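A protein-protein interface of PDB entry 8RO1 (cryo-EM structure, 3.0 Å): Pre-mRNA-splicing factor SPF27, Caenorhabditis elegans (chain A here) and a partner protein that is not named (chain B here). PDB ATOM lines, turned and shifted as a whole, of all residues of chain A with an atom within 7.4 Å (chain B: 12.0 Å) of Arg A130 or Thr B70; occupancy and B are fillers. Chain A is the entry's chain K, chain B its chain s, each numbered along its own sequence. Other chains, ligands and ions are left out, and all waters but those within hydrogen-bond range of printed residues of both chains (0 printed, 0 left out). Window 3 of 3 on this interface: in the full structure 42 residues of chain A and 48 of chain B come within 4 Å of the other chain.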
ATOM      1  N   ASN A 124      18.186  20.932  11.791  1.00  0.00           N
ATOM      2  CA  ASN A 124      18.454  20.692  10.374  1.00  0.00           C
ATOM      3  C   ASN A 124      17.583  19.586   9.788  1.00  0.00           C
ATOM      4  O   ASN A 124      17.160  19.673   8.631  1.00  0.00           O
ATOM      5  CB  ASN A 124      19.921  20.328  10.185  1.00  0.00           C
ATOM      6  CG  ASN A 124      20.782  21.525   9.926  1.00  0.00           C
ATOM      7  OD1 ASN A 124      20.831  22.039   8.813  1.00  0.00           O
ATOM      8  ND2 ASN A 124      21.463  21.993  10.963  1.00  0.00           N
ATOM      9  N   GLU A 125      17.308  18.534  10.561  1.00  0.00           N
ATOM     10  CA  GLU A 125      16.419  17.470  10.100  1.00  0.00           C
ATOM     11  C   GLU A 125      14.950  17.862  10.121  1.00  0.00           C
ATOM     12  O   GLU A 125      14.198  17.470   9.223  1.00  0.00           O
ATOM     13  CB  GLU A 125      16.623  16.217  10.936  1.00  0.00           C
ATOM     14  CG  GLU A 125      17.803  15.387  10.528  1.00  0.00           C
ATOM     15  CD  GLU A 125      17.599  14.672   9.211  1.00  0.00           C
ATOM     16  OE1 GLU A 125      16.682  13.831   9.123  1.00  0.00           O
ATOM     17  OE2 GLU A 125      18.374  14.940   8.269  1.00  0.00           O
ATOM     18  N   HIS A 126      14.514  18.593  11.147  1.00  0.00           N
ATOM     19  CA  HIS A 126      13.146  19.101  11.160  1.00  0.00           C
ATOM     20  C   HIS A 126      12.876  19.964   9.939  1.00  0.00           C
ATOM     21  O   HIS A 126      11.811  19.865   9.321  1.00  0.00           O
ATOM     22  CB  HIS A 126      12.892  19.893  12.440  1.00  0.00           C
ATOM     23  CG  HIS A 126      12.774  19.047  13.668  1.00  0.00           C
ATOM     24  ND1 HIS A 126      11.822  18.062  13.800  1.00  0.00           N
ATOM     25  CD2 HIS A 126      13.484  19.042  14.818  1.00  0.00           C
ATOM     26  CE1 HIS A 126      11.942  17.495  14.986  1.00  0.00           C
ATOM     27  NE2 HIS A 126      12.947  18.067  15.621  1.00  0.00           N
ATOM     28  N   LEU A 127      13.836  20.804   9.568  1.00  0.00           N
ATOM     29  CA  LEU A 127      13.694  21.590   8.351  1.00  0.00           C
ATOM     30  C   LEU A 127      13.751  20.711   7.110  1.00  0.00           C
ATOM     31  O   LEU A 127      13.039  20.965   6.135  1.00  0.00           O
ATOM     32  CB  LEU A 127      14.784  22.653   8.295  1.00  0.00           C
ATOM     33  CG  LEU A 127      14.663  23.789   9.309  1.00  0.00           C
ATOM     34  CD1 LEU A 127      15.955  24.581   9.363  1.00  0.00           C
ATOM     35  CD2 LEU A 127      13.497  24.699   8.988  1.00  0.00           C
ATOM     36  N   LEU A 128      14.598  19.680   7.115  1.00  0.00           N
ATOM     37  CA  LEU A 128      14.647  18.765   5.977  1.00  0.00           C
ATOM     38  C   LEU A 128      13.336  18.011   5.804  1.00  0.00           C
ATOM     39  O   LEU A 128      12.829  17.879   4.686  1.00  0.00           O
ATOM     40  CB  LEU A 128      15.810  17.787   6.143  1.00  0.00           C
ATOM     41  CG  LEU A 128      15.983  16.700   5.073  1.00  0.00           C
ATOM     42  CD1 LEU A 128      16.218  17.301   3.706  1.00  0.00           C
ATOM     43  CD2 LEU A 128      17.128  15.794   5.433  1.00  0.00           C
ATOM     44  N   MET A 129      12.776  17.488   6.894  1.00  0.00           N
ATOM     45  CA  MET A 129      11.474  16.833   6.809  1.00  0.00           C
ATOM     46  C   MET A 129      10.378  17.815   6.432  1.00  0.00           C
ATOM     47  O   MET A 129       9.428  17.457   5.728  1.00  0.00           O
ATOM     48  CB  MET A 129      11.135  16.152   8.131  1.00  0.00           C
ATOM     49  CG  MET A 129      11.991  14.943   8.445  1.00  0.00           C
ATOM     50  SD  MET A 129      11.784  13.549   7.320  1.00  0.00           S
ATOM     51  CE  MET A 129      10.121  13.026   7.725  1.00  0.00           C
ATOM     52  N   ARG A 130      10.482  19.053   6.909  1.00  0.00           N
ATOM     53  CA  ARG A 130       9.557  20.098   6.489  1.00  0.00           C
ATOM     54  C   ARG A 130       9.592  20.312   4.982  1.00  0.00           C
ATOM     55  O   ARG A 130       8.542  20.424   4.343  1.00  0.00           O
ATOM     56  CB  ARG A 130       9.897  21.388   7.234  1.00  0.00           C
ATOM     57  CG  ARG A 130       8.972  22.556   7.012  1.00  0.00           C
ATOM     58  CD  ARG A 130       9.472  23.750   7.796  1.00  0.00           C
ATOM     59  NE  ARG A 130       8.616  24.916   7.633  1.00  0.00           N
ATOM     60  CZ  ARG A 130       8.875  26.124   8.118  1.00  0.00           C
ATOM     61  NH1 ARG A 130       8.005  27.104   7.901  1.00  0.00           N
ATOM     62  NH2 ARG A 130       9.977  26.384   8.806  1.00  0.00           N
ATOM     63  N   GLN A 131      10.789  20.355   4.395  1.00  0.00           N
ATOM     64  CA  GLN A 131      10.911  20.510   2.948  1.00  0.00           C
ATOM     65  C   GLN A 131      10.247  19.364   2.196  1.00  0.00           C
ATOM     66  O   GLN A 131       9.544  19.586   1.205  1.00  0.00           O
ATOM     67  CB  GLN A 131      12.384  20.626   2.565  1.00  0.00           C
ATOM     68  CG  GLN A 131      12.983  21.976   2.915  1.00  0.00           C
ATOM     69  CD  GLN A 131      14.431  22.102   2.496  1.00  0.00           C
ATOM     70  OE1 GLN A 131      15.031  21.146   2.012  1.00  0.00           O
ATOM     71  NE2 GLN A 131      15.010  23.280   2.703  1.00  0.00           N
ATOM     72  N   ILE A 132      10.486  18.125   2.626  1.00  0.00           N
ATOM     73  CA  ILE A 132       9.854  16.979   1.978  1.00  0.00           C
ATOM     74  C   ILE A 132       8.341  17.050   2.122  1.00  0.00           C
ATOM     75  O   ILE A 132       7.600  16.760   1.176  1.00  0.00           O
ATOM     76  CB  ILE A 132      10.418  15.651   2.526  1.00  0.00           C
ATOM     77  CG1 ILE A 132      11.920  15.529   2.224  1.00  0.00           C
ATOM     78  CG2 ILE A 132       9.669  14.460   1.907  1.00  0.00           C
ATOM     79  CD1 ILE A 132      12.645  14.428   2.990  1.00  0.00           C
ATOM     80  N   ASN A 133       7.856  17.403   3.310  1.00  0.00           N
ATOM     81  CA  ASN A 133       6.418  17.539   3.518  1.00  0.00           C
ATOM     82  C   ASN A 133       5.827  18.646   2.661  1.00  0.00           C
ATOM     83  O   ASN A 133       4.778  18.463   2.036  1.00  0.00           O
ATOM     84  CB  ASN A 133       6.118  17.806   4.990  1.00  0.00           C
ATOM     85  CG  ASN A 133       6.263  16.578   5.847  1.00  0.00           C
ATOM     86  OD1 ASN A 133       6.177  15.452   5.366  1.00  0.00           O
ATOM     87  ND2 ASN A 133       6.462  16.788   7.141  1.00  0.00           N
ATOM     88  N   LEU A 134       6.490  19.801   2.609  1.00  0.00           N
ATOM     89  CA  LEU A 134       5.982  20.902   1.798  1.00  0.00           C
ATOM     90  C   LEU A 134       5.965  20.553   0.317  1.00  0.00           C
ATOM     91  O   LEU A 134       5.006  20.880  -0.389  1.00  0.00           O
ATOM     92  CB  LEU A 134       6.835  22.149   2.024  1.00  0.00           C
ATOM     93  CG  LEU A 134       6.732  22.864   3.371  1.00  0.00           C
ATOM     94  CD1 LEU A 134       7.891  23.828   3.574  1.00  0.00           C
ATOM     95  CD2 LEU A 134       5.436  23.610   3.500  1.00  0.00           C
ATOM     96  N   GLU A 135       6.998  19.869  -0.171  1.00  0.00           N
ATOM     97  CA  GLU A 135       7.016  19.490  -1.580  1.00  0.00           C
ATOM     98  C   GLU A 135       5.931  18.477  -1.912  1.00  0.00           C
ATOM     99  O   GLU A 135       5.323  18.543  -2.984  1.00  0.00           O
ATOM    100  CB  GLU A 135       8.387  18.929  -1.938  1.00  0.00           C
ATOM    101  CG  GLU A 135       9.461  19.986  -2.057  1.00  0.00           C
ATOM    102  CD  GLU A 135      10.846  19.393  -2.174  1.00  0.00           C
ATOM    103  OE1 GLU A 135      10.952  18.168  -2.396  1.00  0.00           O
ATOM    104  OE2 GLU A 135      11.830  20.147  -2.031  1.00  0.00           O
ATOM    105  N   LEU A 136       5.669  17.534  -1.010  1.00  0.00           N
ATOM    106  CA  LEU A 136       4.524  16.649  -1.178  1.00  0.00           C
ATOM    107  C   LEU A 136       3.213  17.395  -1.018  1.00  0.00           C
ATOM    108  O   LEU A 136       2.241  17.114  -1.727  1.00  0.00           O
ATOM    109  CB  LEU A 136       4.606  15.510  -0.175  1.00  0.00           C
ATOM    110  CG  LEU A 136       5.734  14.521  -0.446  1.00  0.00           C
ATOM    111  CD1 LEU A 136       6.094  13.757   0.797  1.00  0.00           C
ATOM    112  CD2 LEU A 136       5.314  13.550  -1.531  1.00  0.00           C
ATOM    113  N   MET A 137       3.167  18.346  -0.086  1.00  0.00           N
ATOM    114  CA  MET A 137       1.960  19.137   0.108  1.00  0.00           C
ATOM    115  C   MET A 137       1.632  19.933  -1.148  1.00  0.00           C
ATOM    116  O   MET A 137       0.460  20.096  -1.504  1.00  0.00           O
ATOM    117  CB  MET A 137       2.133  20.050   1.323  1.00  0.00           C
ATOM    118  CG  MET A 137       0.844  20.666   1.799  1.00  0.00           C
ATOM    119  SD  MET A 137       0.954  21.688   3.266  1.00  0.00           S
ATOM    120  CE  MET A 137      -0.776  21.748   3.718  1.00  0.00           C
ATOM    121  N   SER B  62      -6.818   9.829   6.521  1.00  0.00           N
ATOM    122  CA  SER B  62      -6.278  10.972   7.250  1.00  0.00           C
ATOM    123  C   SER B  62      -6.770  12.294   6.671  1.00  0.00           C
ATOM    124  O   SER B  62      -6.909  12.453   5.456  1.00  0.00           O
ATOM    125  CB  SER B  62      -4.748  10.932   7.219  1.00  0.00           C
ATOM    126  OG  SER B  62      -4.192  11.989   7.983  1.00  0.00           O
ATOM    127  N   ALA B  63      -7.034  13.246   7.563  1.00  0.00           N
ATOM    128  CA  ALA B  63      -7.248  14.620   7.147  1.00  0.00           C
ATOM    129  C   ALA B  63      -5.969  15.183   6.522  1.00  0.00           C
ATOM    130  O   ALA B  63      -4.863  14.781   6.897  1.00  0.00           O
ATOM    131  CB  ALA B  63      -7.666  15.481   8.335  1.00  0.00           C
ATOM    132  N   PRO B  64      -6.078  16.105   5.559  1.00  0.00           N
ATOM    133  CA  PRO B  64      -4.879  16.811   5.093  1.00  0.00           C
ATOM    134  C   PRO B  64      -4.233  17.632   6.194  1.00  0.00           C
ATOM    135  O   PRO B  64      -4.888  18.064   7.142  1.00  0.00           O
ATOM    136  CB  PRO B  64      -5.411  17.717   3.980  1.00  0.00           C
ATOM    137  CG  PRO B  64      -6.661  17.106   3.557  1.00  0.00           C
ATOM    138  CD  PRO B  64      -7.256  16.482   4.759  1.00  0.00           C
ATOM    139  N   ARG B  65      -2.928  17.845   6.058  1.00  0.00           N
ATOM    140  CA  ARG B  65      -2.246  18.755   6.961  1.00  0.00           C
ATOM    141  C   ARG B  65      -2.703  20.184   6.725  1.00  0.00           C
ATOM    142  O   ARG B  65      -2.956  20.601   5.593  1.00  0.00           O
ATOM    143  CB  ARG B  65      -0.737  18.694   6.769  1.00  0.00           C
ATOM    144  CG  ARG B  65      -0.131  17.348   7.001  1.00  0.00           C
ATOM    145  CD  ARG B  65       1.370  17.439   7.022  1.00  0.00           C
ATOM    146  NE  ARG B  65       1.947  16.100   7.081  1.00  0.00           N
ATOM    147  CZ  ARG B  65       2.994  15.721   7.805  1.00  0.00           C
ATOM    148  NH1 ARG B  65       3.416  14.466   7.713  1.00  0.00           N
ATOM    149  NH2 ARG B  65       3.603  16.539   8.650  1.00  0.00           N
ATOM    150  N   ASN B  66      -2.769  20.949   7.805  1.00  0.00           N
ATOM    151  CA  ASN B  66      -2.640  22.389   7.694  1.00  0.00           C
ATOM    152  C   ASN B  66      -1.216  22.738   7.288  1.00  0.00           C
ATOM    153  O   ASN B  66      -0.279  21.971   7.516  1.00  0.00           O
ATOM    154  CB  ASN B  66      -2.999  23.059   9.015  1.00  0.00           C
ATOM    155  CG  ASN B  66      -4.459  22.884   9.376  1.00  0.00           C
ATOM    156  OD1 ASN B  66      -5.291  22.579   8.522  1.00  0.00           O
ATOM    157  ND2 ASN B  66      -4.779  23.072  10.650  1.00  0.00           N
ATOM    158  N   VAL B  67      -1.066  23.899   6.652  1.00  0.00           N
ATOM    159  CA  VAL B  67       0.247  24.334   6.180  1.00  0.00           C
ATOM    160  C   VAL B  67       1.211  24.493   7.350  1.00  0.00           C
ATOM    161  O   VAL B  67       2.410  24.224   7.214  1.00  0.00           O
ATOM    162  CB  VAL B  67       0.125  25.640   5.362  1.00  0.00           C
ATOM    163  CG1 VAL B  67       1.488  26.047   4.736  1.00  0.00           C
ATOM    164  CG2 VAL B  67      -0.983  25.523   4.291  1.00  0.00           C
ATOM    165  N   SER B  68       0.717  24.933   8.507  1.00  0.00           N
ATOM    166  CA  SER B  68       1.547  24.944   9.704  1.00  0.00           C
ATOM    167  C   SER B  68       1.848  23.550  10.240  1.00  0.00           C
ATOM    168  O   SER B  68       2.791  23.398  11.018  1.00  0.00           O
ATOM    169  CB  SER B  68       0.868  25.773  10.794  1.00  0.00           C
ATOM    170  OG  SER B  68      -0.444  25.303  11.039  1.00  0.00           O
ATOM    171  N   GLY B  69       1.088  22.535   9.848  1.00  0.00           N
ATOM    172  CA  GLY B  69       1.333  21.187  10.309  1.00  0.00           C
ATOM    173  C   GLY B  69       2.393  20.422   9.553  1.00  0.00           C
ATOM    174  O   GLY B  69       2.544  19.220   9.779  1.00  0.00           O
ATOM    175  N   THR B  70       3.125  21.069   8.649  1.00  0.00           N
ATOM    176  CA  THR B  70       4.123  20.381   7.842  1.00  0.00           C
ATOM    177  C   THR B  70       5.436  20.127   8.562  1.00  0.00           C
ATOM    178  O   THR B  70       6.313  19.492   7.969  1.00  0.00           O
ATOM    179  CB  THR B  70       4.421  21.195   6.587  1.00  0.00           C
ATOM    180  OG1 THR B  70       4.748  22.538   6.963  1.00  0.00           O
ATOM    181  CG2 THR B  70       3.225  21.222   5.681  1.00  0.00           C
ATOM    182  N   SER B  71       5.598  20.585   9.801  1.00  0.00           N
ATOM    183  CA  SER B  71       6.822  20.385  10.556  1.00  0.00           C
ATOM    184  C   SER B  71       6.488  19.736  11.887  1.00  0.00           C
ATOM    185  O   SER B  71       5.419  19.967  12.456  1.00  0.00           O
ATOM    186  CB  SER B  71       7.535  21.714  10.777  1.00  0.00           C
ATOM    187  OG  SER B  71       8.831  21.520  11.296  1.00  0.00           O
ATOM    188  N   ILE B  72       7.421  18.927  12.383  1.00  0.00           N
ATOM    189  CA  ILE B  72       7.173  18.177  13.614  1.00  0.00           C
ATOM    190  C   ILE B  72       6.990  19.096  14.815  1.00  0.00           C
ATOM    191  O   ILE B  72       6.026  18.898  15.572  1.00  0.00           O
ATOM    192  CB  ILE B  72       8.261  17.106  13.817  1.00  0.00           C
ATOM    193  CG1 ILE B  72       8.044  15.896  12.885  1.00  0.00           C
ATOM    194  CG2 ILE B  72       8.352  16.632  15.289  1.00  0.00           C
ATOM    195  CD1 ILE B  72       8.467  16.087  11.441  1.00  0.00           C
ATOM    196  N   PRO B  73       7.852  20.085  15.067  1.00  0.00           N
ATOM    197  CA  PRO B  73       7.576  20.997  16.183  1.00  0.00           C
ATOM    198  C   PRO B  73       6.303  21.797  16.028  1.00  0.00           C
ATOM    199  O   PRO B  73       5.643  22.070  17.035  1.00  0.00           O
ATOM    200  CB  PRO B  73       8.806  21.912  16.198  1.00  0.00           C
ATOM    201  CG  PRO B  73       9.846  21.156  15.530  1.00  0.00           C
ATOM    202  CD  PRO B  73       9.158  20.390  14.466  1.00  0.00           C
ATOM    203  N   SER B  74       5.934  22.196  14.813  1.00  0.00           N
ATOM    204  CA  SER B  74       4.677  22.911  14.665  1.00  0.00           C
ATOM    205  C   SER B  74       3.472  21.994  14.791  1.00  0.00           C
ATOM    206  O   SER B  74       2.384  22.473  15.122  1.00  0.00           O
ATOM    207  CB  SER B  74       4.644  23.632  13.320  1.00  0.00           C
ATOM    208  OG  SER B  74       4.689  22.722  12.237  1.00  0.00           O
ATOM    209  N   LEU B  75       3.628  20.693  14.535  1.00  0.00           N
ATOM    210  CA  LEU B  75       2.601  19.741  14.942  1.00  0.00           C
ATOM    211  C   LEU B  75       2.490  19.645  16.455  1.00  0.00           C
ATOM    212  O   LEU B  75       1.384  19.549  16.994  1.00  0.00           O
ATOM    213  CB  LEU B  75       2.895  18.364  14.357  1.00  0.00           C
ATOM    214  CG  LEU B  75       2.601  18.130  12.879  1.00  0.00           C
ATOM    215  CD1 LEU B  75       3.136  16.779  12.466  1.00  0.00           C
ATOM    216  CD2 LEU B  75       1.127  18.196  12.593  1.00  0.00           C
ATOM    217  N   LEU B  76       3.621  19.668  17.162  1.00  0.00           N
ATOM    218  CA  LEU B  76       3.568  19.679  18.619  1.00  0.00           C
ATOM    219  C   LEU B  76       2.947  20.964  19.148  1.00  0.00           C
ATOM    220  O   LEU B  76       2.215  20.941  20.141  1.00  0.00           O
ATOM    221  CB  LEU B  76       4.965  19.482  19.198  1.00  0.00           C
ATOM    222  CG  LEU B  76       5.673  18.158  18.898  1.00  0.00           C
ATOM    223  CD1 LEU B  76       7.038  18.158  19.538  1.00  0.00           C
ATOM    224  CD2 LEU B  76       4.878  16.959  19.366  1.00  0.00           C
ATOM    225  N   LYS B  77       3.241  22.098  18.513  1.00  0.00           N
ATOM    226  CA  LYS B  77       2.545  23.335  18.843  1.00  0.00           C
ATOM    227  C   LYS B  77       1.059  23.196  18.569  1.00  0.00           C
ATOM    228  O   LYS B  77       0.219  23.581  19.386  1.00  0.00           O
ATOM    229  CB  LYS B  77       3.124  24.499  18.039  1.00  0.00           C
ATOM    230  CG  LYS B  77       2.335  25.798  18.145  1.00  0.00           C
ATOM    231  CD  LYS B  77       3.135  26.979  17.622  1.00  0.00           C
ATOM    232  CE  LYS B  77       2.251  28.200  17.411  1.00  0.00           C
ATOM    233  NZ  LYS B  77       1.539  28.618  18.651  1.00  0.00           N
ATOM    234  N   MET B  78       0.725  22.656  17.401  1.00  0.00           N
ATOM    235  CA  MET B  78      -0.667  22.441  17.037  1.00  0.00           C
ATOM    236  C   MET B  78      -1.342  21.450  17.976  1.00  0.00           C
ATOM    237  O   MET B  78      -2.507  21.626  18.341  1.00  0.00           O
ATOM    238  CB  MET B  78      -0.725  21.954  15.594  1.00  0.00           C
ATOM    239  CG  MET B  78      -2.106  21.870  14.981  1.00  0.00           C
ATOM    240  SD  MET B  78      -2.090  21.292  13.268  1.00  0.00           S
ATOM    241  CE  MET B  78      -1.148  22.557  12.417  1.00  0.00           C
ATOM    242  N   LEU B  79      -0.632  20.396  18.371  1.00  0.00           N
ATOM    243  CA  LEU B  79      -1.198  19.442  19.318  1.00  0.00           C
ATOM    244  C   LEU B  79      -1.426  20.076  20.684  1.00  0.00           C
ATOM    245  O   LEU B  79      -2.438  19.800  21.336  1.00  0.00           O
ATOM    246  CB  LEU B  79      -0.290  18.218  19.422  1.00  0.00           C
ATOM    247  CG  LEU B  79      -0.632  17.097  20.400  1.00  0.00           C
ATOM    248  CD1 LEU B  79      -1.939  16.439  20.022  1.00  0.00           C
ATOM    249  CD2 LEU B  79       0.477  16.071  20.397  1.00  0.00           C
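The side-chain amide nitrogen (ND2) of Asn A133 sits at hydrogen-bond distance from the backbone carbonyl oxygen (O) of Thr B70, at 2.8 Å.
The side-chain amide nitrogen of Asn A133 sits close to the guanidinium group of Arg B65 (3.2 Å).
Of the printed residues of chain B, Arg A130 touches Thr B70.
Of chain A, only Arg A130 (3.6 Å), Asn A133 (2.8 Å), Leu A134 (3.7 Å) and Met A137 (3.3 Å) come within 4 Å of Thr B70.
No residue of chain B comes within 4 Å of Leu A128.
No residue of chain B comes within 4 Å of Met A129.
No residue of chain B comes within 4 Å of Gln A131.
Asn A133 touches just these residues of chain B: Arg B65 (3.2 Å) and Thr B70 (2.8 Å).
Of chain B, only Arg B65, Asn B66, Val B67 and Thr B70 come within 4 Å of Met A137.
No residue of chain A comes within 4 Å of Gly B69.
Of the printed residues of chain B, His A126 touches Ser B71 (3.9 Å), Ile B72 (3.7 Å) and Pro B73 (3.6 Å).
Of the printed residues of chain A, Pro B73 touches His A126 (3.6 Å).
Of the printed residues of chain A, Val B67 touches Met A137.
Printed residues of chain A within 4 Å of Arg B65: Asn A133 and Met A137.
Pro B64 touches none of the printed residues of chain A.
Lys B77 touches none of the printed residues of chain A.
The nearest residue of chain A that does not touch Thr B70 is Met A129 (4.3 Å).
The nearest printed residue of chain A that does not touch Arg B65 is Met A129 (6.6 Å).
Of the 18 printed residues of chain B, 7 touch a printed residue of chain A.
Printed residues of chain B that touch a printed residue of chain A: Arg B65, Asn B66, Val B67, Thr B70, Ser B71, Ile B72 and Pro B73.
Hydrophobic or aromatic side chains of chain B within 4 Å of the printed part of chain A: Val B67, Ile B72 and Pro B73.
Of the 14 printed residues of chain A, 5 touch a printed residue of chain B.
Among the printed residues, 11 pairs touch across the chains.
His A126 touches Ser B71 (O to OG, 3.9 Å).
Ile B72 touches His A126.
His A126 touches Pro B73.
CA of Arg A130 touches O of Thr B70, 3.6 Å away.
Leu A134 touches Thr B70.
O of Arg B65 touches CE of Met A137, 3.1 Å away.
C of Asn B66 touches CE of Met A137, 3.7 Å away.
Met A137 touches Val B67 (CE to N, 3.6 Å).
Met A137 touches Thr B70 (SD to CG2, 3.3 Å).
The backbone carbonyl oxygen of Ser B71 lies within hydrogen-bond range of the side-chain hydroxyl of Ser B74 (2.9 Å).
O of Val B67 is in hydrogen-bond range of OG1 of Thr B70.
The backbone carbonyl oxygen (O) of Met A129 lies close to the side-chain amide nitrogen (ND2) of Asn A133 (3.4 Å).
NH2 of Arg B65 is in hydrogen-bond range of O of Gly B69 (3.1 Å).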
